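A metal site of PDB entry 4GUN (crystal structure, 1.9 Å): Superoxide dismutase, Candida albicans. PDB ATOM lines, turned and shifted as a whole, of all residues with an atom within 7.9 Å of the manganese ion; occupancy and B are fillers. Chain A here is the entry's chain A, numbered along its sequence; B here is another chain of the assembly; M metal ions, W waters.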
ATOM      1  N   HIS A  32     -26.363 -12.882  14.919  1.00  0.00           N
ATOM      2  CA  HIS A  32     -25.372 -13.868  14.506  1.00  0.00           C
ATOM      3  C   HIS A  32     -23.958 -13.331  14.523  1.00  0.00           C
ATOM      4  O   HIS A  32     -23.085 -13.937  15.131  1.00  0.00           O
ATOM      5  CB  HIS A  32     -25.740 -14.508  13.153  1.00  0.00           C
ATOM      6  CG  HIS A  32     -25.243 -15.932  13.002  1.00  0.00           C
ATOM      7  ND1 HIS A  32     -25.464 -16.636  11.844  1.00  0.00           N
ATOM      8  CD2 HIS A  32     -24.532 -16.707  13.854  1.00  0.00           C
ATOM      9  CE1 HIS A  32     -24.899 -17.814  12.019  1.00  0.00           C
ATOM     10  NE2 HIS A  32     -24.317 -17.895  13.213  1.00  0.00           N
ATOM     11  N   ILE A  33     -23.750 -12.161  13.925  1.00  0.00           N
ATOM     12  CA  ILE A  33     -22.442 -11.513  13.847  1.00  0.00           C
ATOM     13  C   ILE A  33     -22.067 -10.781  15.149  1.00  0.00           C
ATOM     14  O   ILE A  33     -20.987 -11.017  15.702  1.00  0.00           O
ATOM     15  CB  ILE A  33     -22.368 -10.566  12.592  1.00  0.00           C
ATOM     16  CG1 ILE A  33     -22.668 -11.331  11.276  1.00  0.00           C
ATOM     17  CG2 ILE A  33     -21.006  -9.820  12.534  1.00  0.00           C
ATOM     18  CD1 ILE A  33     -22.988 -10.481  10.063  1.00  0.00           C
ATOM     19  N   HIS A  36     -23.272 -13.601  18.641  1.00  0.00           N
ATOM     20  CA  HIS A  36     -22.644 -14.927  18.545  1.00  0.00           C
ATOM     21  C   HIS A  36     -21.169 -14.950  18.165  1.00  0.00           C
ATOM     22  O   HIS A  36     -20.379 -15.569  18.889  1.00  0.00           O
ATOM     23  CB  HIS A  36     -23.495 -15.943  17.732  1.00  0.00           C
ATOM     24  CG  HIS A  36     -24.840 -16.204  18.317  1.00  0.00           C
ATOM     25  ND1 HIS A  36     -25.036 -17.159  19.302  1.00  0.00           N
ATOM     26  CD2 HIS A  36     -26.028 -15.593  18.063  1.00  0.00           C
ATOM     27  CE1 HIS A  36     -26.326 -17.126  19.588  1.00  0.00           C
ATOM     28  NE2 HIS A  36     -26.967 -16.200  18.869  1.00  0.00           N
ATOM     29  N   HIS A  37     -20.806 -14.345  17.026  1.00  0.00           N
ATOM     30  CA  HIS A  37     -19.401 -14.316  16.610  1.00  0.00           C
ATOM     31  C   HIS A  37     -18.586 -13.513  17.623  1.00  0.00           C
ATOM     32  O   HIS A  37     -17.535 -13.972  18.041  1.00  0.00           O
ATOM     33  CB  HIS A  37     -19.234 -13.772  15.166  1.00  0.00           C
ATOM     34  CG  HIS A  37     -17.874 -13.975  14.550  1.00  0.00           C
ATOM     35  ND1 HIS A  37     -17.705 -13.963  13.176  1.00  0.00           N
ATOM     36  CD2 HIS A  37     -16.663 -14.175  15.140  1.00  0.00           C
ATOM     37  CE1 HIS A  37     -16.416 -14.176  12.975  1.00  0.00           C
ATOM     38  NE2 HIS A  37     -15.754 -14.291  14.134  1.00  0.00           N
ATOM     39  N   TYR A  40     -17.485 -15.629  20.568  1.00  0.00           N
ATOM     40  CA  TYR A  40     -16.331 -16.483  20.268  1.00  0.00           C
ATOM     41  C   TYR A  40     -15.021 -15.658  20.208  1.00  0.00           C
ATOM     42  O   TYR A  40     -13.981 -16.161  20.634  1.00  0.00           O
ATOM     43  CB  TYR A  40     -16.528 -17.293  18.973  1.00  0.00           C
ATOM     44  CG  TYR A  40     -17.774 -18.138  18.955  1.00  0.00           C
ATOM     45  CD1 TYR A  40     -17.962 -19.158  19.881  1.00  0.00           C
ATOM     46  CD2 TYR A  40     -18.726 -17.994  17.939  1.00  0.00           C
ATOM     47  CE1 TYR A  40     -19.105 -19.956  19.862  1.00  0.00           C
ATOM     48  CE2 TYR A  40     -19.885 -18.776  17.927  1.00  0.00           C
ATOM     49  CZ  TYR A  40     -20.066 -19.760  18.875  1.00  0.00           C
ATOM     50  OH  TYR A  40     -21.202 -20.528  18.837  1.00  0.00           O
ATOM     51  N   GLY A  76     -15.256 -21.562  16.667  1.00  0.00           N
ATOM     52  CA  GLY A  76     -16.381 -20.667  16.401  1.00  0.00           C
ATOM     53  C   GLY A  76     -15.984 -19.465  15.555  1.00  0.00           C
ATOM     54  O   GLY A  76     -16.703 -19.111  14.626  1.00  0.00           O
ATOM     55  N   ASN A  79     -15.016 -20.879  11.958  1.00  0.00           N
ATOM     56  CA  ASN A  79     -16.247 -21.302  11.251  1.00  0.00           C
ATOM     57  C   ASN A  79     -17.094 -20.112  10.783  1.00  0.00           C
ATOM     58  O   ASN A  79     -17.503 -20.068   9.615  1.00  0.00           O
ATOM     59  CB  ASN A  79     -17.080 -22.263  12.105  1.00  0.00           C
ATOM     60  CG  ASN A  79     -16.469 -23.647  12.273  1.00  0.00           C
ATOM     61  OD1 ASN A  79     -15.639 -24.090  11.470  1.00  0.00           O
ATOM     62  ND2 ASN A  79     -16.884 -24.375  13.312  1.00  0.00           N
ATOM     63  N   HIS A  80     -17.355 -19.145  11.684  1.00  0.00           N
ATOM     64  CA  HIS A  80     -18.141 -17.962  11.340  1.00  0.00           C
ATOM     65  C   HIS A  80     -17.456 -17.084  10.283  1.00  0.00           C
ATOM     66  O   HIS A  80     -18.122 -16.686   9.344  1.00  0.00           O
ATOM     67  CB  HIS A  80     -18.606 -17.209  12.591  1.00  0.00           C
ATOM     68  CG  HIS A  80     -19.704 -17.956  13.326  1.00  0.00           C
ATOM     69  ND1 HIS A  80     -19.410 -18.902  14.279  1.00  0.00           N
ATOM     70  CD2 HIS A  80     -21.043 -17.905  13.152  1.00  0.00           C
ATOM     71  CE1 HIS A  80     -20.573 -19.366  14.701  1.00  0.00           C
ATOM     72  NE2 HIS A  80     -21.586 -18.777  14.074  1.00  0.00           N
ATOM     73  N   PHE A  83     -17.952 -18.689   7.082  1.00  0.00           N
ATOM     74  CA  PHE A  83     -19.379 -18.546   6.755  1.00  0.00           C
ATOM     75  C   PHE A  83     -19.694 -17.202   6.108  1.00  0.00           C
ATOM     76  O   PHE A  83     -20.228 -17.196   4.987  1.00  0.00           O
ATOM     77  CB  PHE A  83     -20.235 -18.814   8.002  1.00  0.00           C
ATOM     78  CG  PHE A  83     -21.720 -18.978   7.791  1.00  0.00           C
ATOM     79  CD1 PHE A  83     -22.223 -19.950   6.926  1.00  0.00           C
ATOM     80  CD2 PHE A  83     -22.628 -18.238   8.542  1.00  0.00           C
ATOM     81  CE1 PHE A  83     -23.596 -20.135   6.759  1.00  0.00           C
ATOM     82  CE2 PHE A  83     -24.012 -18.434   8.393  1.00  0.00           C
ATOM     83  CZ  PHE A  83     -24.489 -19.361   7.492  1.00  0.00           C
ATOM     84  N   TRP A  84     -19.296 -16.086   6.734  1.00  0.00           N
ATOM     85  CA  TRP A  84     -19.579 -14.759   6.165  1.00  0.00           C
ATOM     86  C   TRP A  84     -18.952 -14.559   4.780  1.00  0.00           C
ATOM     87  O   TRP A  84     -19.570 -13.895   3.928  1.00  0.00           O
ATOM     88  CB  TRP A  84     -19.192 -13.605   7.105  1.00  0.00           C
ATOM     89  CG  TRP A  84     -19.419 -13.790   8.583  1.00  0.00           C
ATOM     90  CD1 TRP A  84     -18.530 -13.527   9.578  1.00  0.00           C
ATOM     91  CD2 TRP A  84     -20.646 -14.192   9.235  1.00  0.00           C
ATOM     92  NE1 TRP A  84     -19.123 -13.739  10.808  1.00  0.00           N
ATOM     93  CE2 TRP A  84     -20.399 -14.190  10.623  1.00  0.00           C
ATOM     94  CE3 TRP A  84     -21.916 -14.609   8.765  1.00  0.00           C
ATOM     95  CZ2 TRP A  84     -21.363 -14.600  11.554  1.00  0.00           C
ATOM     96  CZ3 TRP A  84     -22.871 -14.974   9.697  1.00  0.00           C
ATOM     97  CH2 TRP A  84     -22.577 -15.014  11.065  1.00  0.00           C
ATOM     98  N   GLY A 133     -24.032 -28.006  14.928  1.00  0.00           N
ATOM     99  CA  GLY A 133     -22.962 -28.405  14.021  1.00  0.00           C
ATOM    100  C   GLY A 133     -22.917 -27.666  12.712  1.00  0.00           C
ATOM    101  O   GLY A 133     -23.582 -26.648  12.519  1.00  0.00           O
ATOM    102  N   TRP A 134     -22.031 -28.141  11.830  1.00  0.00           N
ATOM    103  CA  TRP A 134     -21.747 -27.548  10.521  1.00  0.00           C
ATOM    104  C   TRP A 134     -21.611 -28.626   9.504  1.00  0.00           C
ATOM    105  O   TRP A 134     -21.292 -29.763   9.852  1.00  0.00           O
ATOM    106  CB  TRP A 134     -20.357 -26.829  10.572  1.00  0.00           C
ATOM    107  CG  TRP A 134     -20.320 -25.613  11.439  1.00  0.00           C
ATOM    108  CD1 TRP A 134     -20.265 -25.579  12.797  1.00  0.00           C
ATOM    109  CD2 TRP A 134     -20.376 -24.250  11.008  1.00  0.00           C
ATOM    110  NE1 TRP A 134     -20.344 -24.287  13.251  1.00  0.00           N
ATOM    111  CE2 TRP A 134     -20.424 -23.450  12.170  1.00  0.00           C
ATOM    112  CE3 TRP A 134     -20.395 -23.627   9.749  1.00  0.00           C
ATOM    113  CZ2 TRP A 134     -20.471 -22.049  12.108  1.00  0.00           C
ATOM    114  CZ3 TRP A 134     -20.469 -22.243   9.692  1.00  0.00           C
ATOM    115  CH2 TRP A 134     -20.500 -21.469  10.858  1.00  0.00           C
ATOM    116  N   ASN A 154     -20.941 -28.928  17.039  1.00  0.00           N
ATOM    117  CA  ASN A 154     -20.670 -27.702  17.781  1.00  0.00           C
ATOM    118  C   ASN A 154     -19.773 -26.730  17.011  1.00  0.00           C
ATOM    119  O   ASN A 154     -20.148 -26.320  15.917  1.00  0.00           O
ATOM    120  CB  ASN A 154     -20.118 -28.035  19.196  1.00  0.00           C
ATOM    121  CG  ASN A 154     -21.094 -28.837  20.029  1.00  0.00           C
ATOM    122  OD1 ASN A 154     -22.301 -28.775  19.810  1.00  0.00           O
ATOM    123  ND2 ASN A 154     -20.602 -29.597  21.000  1.00  0.00           N
ATOM    124  N   GLN A 155     -18.605 -26.364  17.583  1.00  0.00           N
ATOM    125  CA  GLN A 155     -17.663 -25.467  16.895  1.00  0.00           C
ATOM    126  C   GLN A 155     -16.420 -26.188  16.396  1.00  0.00           C
ATOM    127  O   GLN A 155     -15.414 -25.549  16.104  1.00  0.00           O
ATOM    128  CB  GLN A 155     -17.354 -24.168  17.664  1.00  0.00           C
ATOM    129  CG  GLN A 155     -18.544 -23.198  17.832  1.00  0.00           C
ATOM    130  CD  GLN A 155     -19.252 -22.782  16.557  1.00  0.00           C
ATOM    131  OE1 GLN A 155     -18.742 -22.894  15.428  1.00  0.00           O
ATOM    132  NE2 GLN A 155     -20.459 -22.283  16.699  1.00  0.00           N
ATOM    133  N   ASP A 170     -23.544 -23.264   8.461  1.00  0.00           N
ATOM    134  CA  ASP A 170     -23.922 -23.265   9.864  1.00  0.00           C
ATOM    135  C   ASP A 170     -25.302 -23.923  10.050  1.00  0.00           C
ATOM    136  O   ASP A 170     -26.296 -23.436   9.521  1.00  0.00           O
ATOM    137  CB  ASP A 170     -23.954 -21.829  10.417  1.00  0.00           C
ATOM    138  CG  ASP A 170     -23.940 -21.723  11.930  1.00  0.00           C
ATOM    139  OD1 ASP A 170     -23.983 -22.774  12.601  1.00  0.00           O
ATOM    140  OD2 ASP A 170     -23.843 -20.619  12.443  1.00  0.00           O
ATOM    141  N   ALA A 171     -25.348 -25.019  10.843  1.00  0.00           N
ATOM    142  CA  ALA A 171     -26.593 -25.727  11.160  1.00  0.00           C
ATOM    143  C   ALA A 171     -27.043 -25.505  12.626  1.00  0.00           C
ATOM    144  O   ALA A 171     -28.021 -26.139  13.036  1.00  0.00           O
ATOM    145  CB  ALA A 171     -26.440 -27.218  10.867  1.00  0.00           C
ATOM    146  N   TRP A 172     -26.343 -24.621  13.420  1.00  0.00           N
ATOM    147  CA  TRP A 172     -26.792 -24.301  14.803  1.00  0.00           C
ATOM    148  C   TRP A 172     -28.192 -23.669  14.730  1.00  0.00           C
ATOM    149  O   TRP A 172     -28.481 -22.960  13.761  1.00  0.00           O
ATOM    150  CB  TRP A 172     -25.851 -23.310  15.513  1.00  0.00           C
ATOM    151  CG  TRP A 172     -24.586 -23.891  16.078  1.00  0.00           C
ATOM    152  CD1 TRP A 172     -23.600 -24.535  15.393  1.00  0.00           C
ATOM    153  CD2 TRP A 172     -24.092 -23.716  17.423  1.00  0.00           C
ATOM    154  NE1 TRP A 172     -22.543 -24.820  16.227  1.00  0.00           N
ATOM    155  CE2 TRP A 172     -22.814 -24.318  17.481  1.00  0.00           C
ATOM    156  CE3 TRP A 172     -24.617 -23.108  18.592  1.00  0.00           C
ATOM    157  CZ2 TRP A 172     -22.078 -24.381  18.675  1.00  0.00           C
ATOM    158  CZ3 TRP A 172     -23.878 -23.172  19.766  1.00  0.00           C
ATOM    159  CH2 TRP A 172     -22.619 -23.791  19.790  1.00  0.00           C
ATOM    160  N   GLU A 173     -29.073 -23.951  15.706  1.00  0.00           N
ATOM    161  CA  GLU A 173     -30.456 -23.434  15.710  1.00  0.00           C
ATOM    162  C   GLU A 173     -30.521 -21.905  15.622  1.00  0.00           C
ATOM    163  O   GLU A 173     -31.382 -21.395  14.926  1.00  0.00           O
ATOM    164  CB  GLU A 173     -31.264 -23.983  16.889  1.00  0.00           C
ATOM    165  CG  GLU A 173     -31.549 -25.479  16.782  1.00  0.00           C
ATOM    166  CD  GLU A 173     -32.346 -26.048  17.934  1.00  0.00           C
ATOM    167  OE1 GLU A 173     -31.977 -25.773  19.088  1.00  0.00           O
ATOM    168  OE2 GLU A 173     -33.354 -26.745  17.686  1.00  0.00           O
ATOM    169  N   HIS A 174     -29.560 -21.185  16.227  1.00  0.00           N
ATOM    170  CA  HIS A 174     -29.486 -19.723  16.169  1.00  0.00           C
ATOM    171  C   HIS A 174     -29.311 -19.195  14.757  1.00  0.00           C
ATOM    172  O   HIS A 174     -29.641 -18.045  14.498  1.00  0.00           O
ATOM    173  CB  HIS A 174     -28.381 -19.152  17.092  1.00  0.00           C
ATOM    174  CG  HIS A 174     -26.959 -19.428  16.685  1.00  0.00           C
ATOM    175  ND1 HIS A 174     -26.079 -20.087  17.540  1.00  0.00           N
ATOM    176  CD2 HIS A 174     -26.279 -19.050  15.583  1.00  0.00           C
ATOM    177  CE1 HIS A 174     -24.917 -20.125  16.901  1.00  0.00           C
ATOM    178  NE2 HIS A 174     -24.992 -19.510  15.723  1.00  0.00           N
ATOM    179  N   ALA A 175     -28.778 -20.021  13.838  1.00  0.00           N
ATOM    180  CA  ALA A 175     -28.563 -19.616  12.446  1.00  0.00           C
ATOM    181  C   ALA A 175     -29.865 -19.455  11.624  1.00  0.00           C
ATOM    182  O   ALA A 175     -29.852 -18.789  10.575  1.00  0.00           O
ATOM    183  CB  ALA A 175     -27.622 -20.612  11.767  1.00  0.00           C
ATOM    184  N   TYR A 176     -30.960 -20.075  12.072  1.00  0.00           N
ATOM    185  CA  TYR A 176     -32.213 -20.031  11.323  1.00  0.00           C
ATOM    186  C   TYR A 176     -33.476 -19.831  12.143  1.00  0.00           C
ATOM    187  O   TYR A 176     -34.494 -19.415  11.569  1.00  0.00           O
ATOM    188  CB  TYR A 176     -32.332 -21.327  10.502  1.00  0.00           C
ATOM    189  CG  TYR A 176     -32.366 -22.581  11.341  1.00  0.00           C
ATOM    190  CD1 TYR A 176     -33.572 -23.093  11.826  1.00  0.00           C
ATOM    191  CD2 TYR A 176     -31.198 -23.290  11.613  1.00  0.00           C
ATOM    192  CE1 TYR A 176     -33.603 -24.246  12.624  1.00  0.00           C
ATOM    193  CE2 TYR A 176     -31.218 -24.463  12.383  1.00  0.00           C
ATOM    194  CZ  TYR A 176     -32.426 -24.933  12.877  1.00  0.00           C
ATOM    195  OH  TYR A 176     -32.477 -26.063  13.639  1.00  0.00           O
ATOM    196  N   TYR A 187     -34.500 -23.811   5.621  1.00  0.00           N
ATOM    197  CA  TYR A 187     -33.313 -22.987   5.700  1.00  0.00           C
ATOM    198  C   TYR A 187     -32.210 -23.623   4.844  1.00  0.00           C
ATOM    199  O   TYR A 187     -31.605 -22.914   4.039  1.00  0.00           O
ATOM    200  CB  TYR A 187     -32.878 -22.871   7.156  1.00  0.00           C
ATOM    201  CG  TYR A 187     -31.443 -22.440   7.363  1.00  0.00           C
ATOM    202  CD1 TYR A 187     -31.028 -21.157   7.051  1.00  0.00           C
ATOM    203  CD2 TYR A 187     -30.530 -23.283   7.983  1.00  0.00           C
ATOM    204  CE1 TYR A 187     -29.720 -20.724   7.314  1.00  0.00           C
ATOM    205  CE2 TYR A 187     -29.231 -22.872   8.264  1.00  0.00           C
ATOM    206  CZ  TYR A 187     -28.831 -21.593   7.929  1.00  0.00           C
ATOM    207  OH  TYR A 187     -27.547 -21.178   8.177  1.00  0.00           O
ATOM    208  N   GLU B 173     -30.952 -24.436  22.005  1.00  0.00           N
ATOM    209  CA  GLU B 173     -31.386 -23.060  21.649  1.00  0.00           C
ATOM    210  C   GLU B 173     -32.892 -22.941  21.429  1.00  0.00           C
ATOM    211  O   GLU B 173     -33.483 -21.928  21.813  1.00  0.00           O
ATOM    212  CB  GLU B 173     -30.565 -22.464  20.502  1.00  0.00           C
ATOM    213  CG  GLU B 173     -29.098 -22.346  20.864  1.00  0.00           C
ATOM    214  CD  GLU B 173     -28.185 -21.857  19.768  1.00  0.00           C
ATOM    215  OE1 GLU B 173     -28.255 -22.406  18.649  1.00  0.00           O
ATOM    216  OE2 GLU B 173     -27.367 -20.948  20.045  1.00  0.00           O
HETATM  217 MN    MN M   1     -23.523 -19.655  14.179  1.00  0.00          MN
HETATM  218  O   HOH W   1     -22.782 -21.573  14.831  1.00  0.00           O
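ND1 of His 80 is in hydrogen-bond range of O of Gly 76 (2.7 Å).
The backbone NH (N) of His 37 sits at hydrogen-bond distance from the backbone carbonyl oxygen (O) of His 32 (3.0 Å).
The side-chain hydroxyl (OH) of Tyr 187 lies within hydrogen-bond range of the backbone carbonyl oxygen (O) of Asp 170.
The side-chain carboxylate (OD1) of Asp 170 lies within hydrogen-bond range of the backbone NH (N) of Trp 172.
The indole nitrogen of Trp 84 sits close to the backbone carbonyl oxygen of His 80, at 3.4 Å.
A ring nitrogen (ND1) of His 174 lies within hydrogen-bond range of the side-chain carboxylate of Glu 173 of chain B, 2.9 Å away.
Within 4 Å of the manganese ion: His 32, His 80, Asp 170 and His 174.
The nearest printed residue that does not touch the manganese ion is Trp 134 (4.4 Å).
Water W1 lies within hydrogen-bond range of OD1 of Asp 170 (2.8 Å) and NE2 of Gln 155 (3.1 Å).
OD2 of Asp 170 binds the manganese ion, 2.0 Å away.
NE2 of His 80 binds the manganese ion, at 2.1 Å.
A ring nitrogen (NE2) of His 174 is bound to the manganese ion.
The manganese ion is bound by water W1 (2.2 Å).
NE2 of His 32 binds the manganese ion (2.2 Å).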
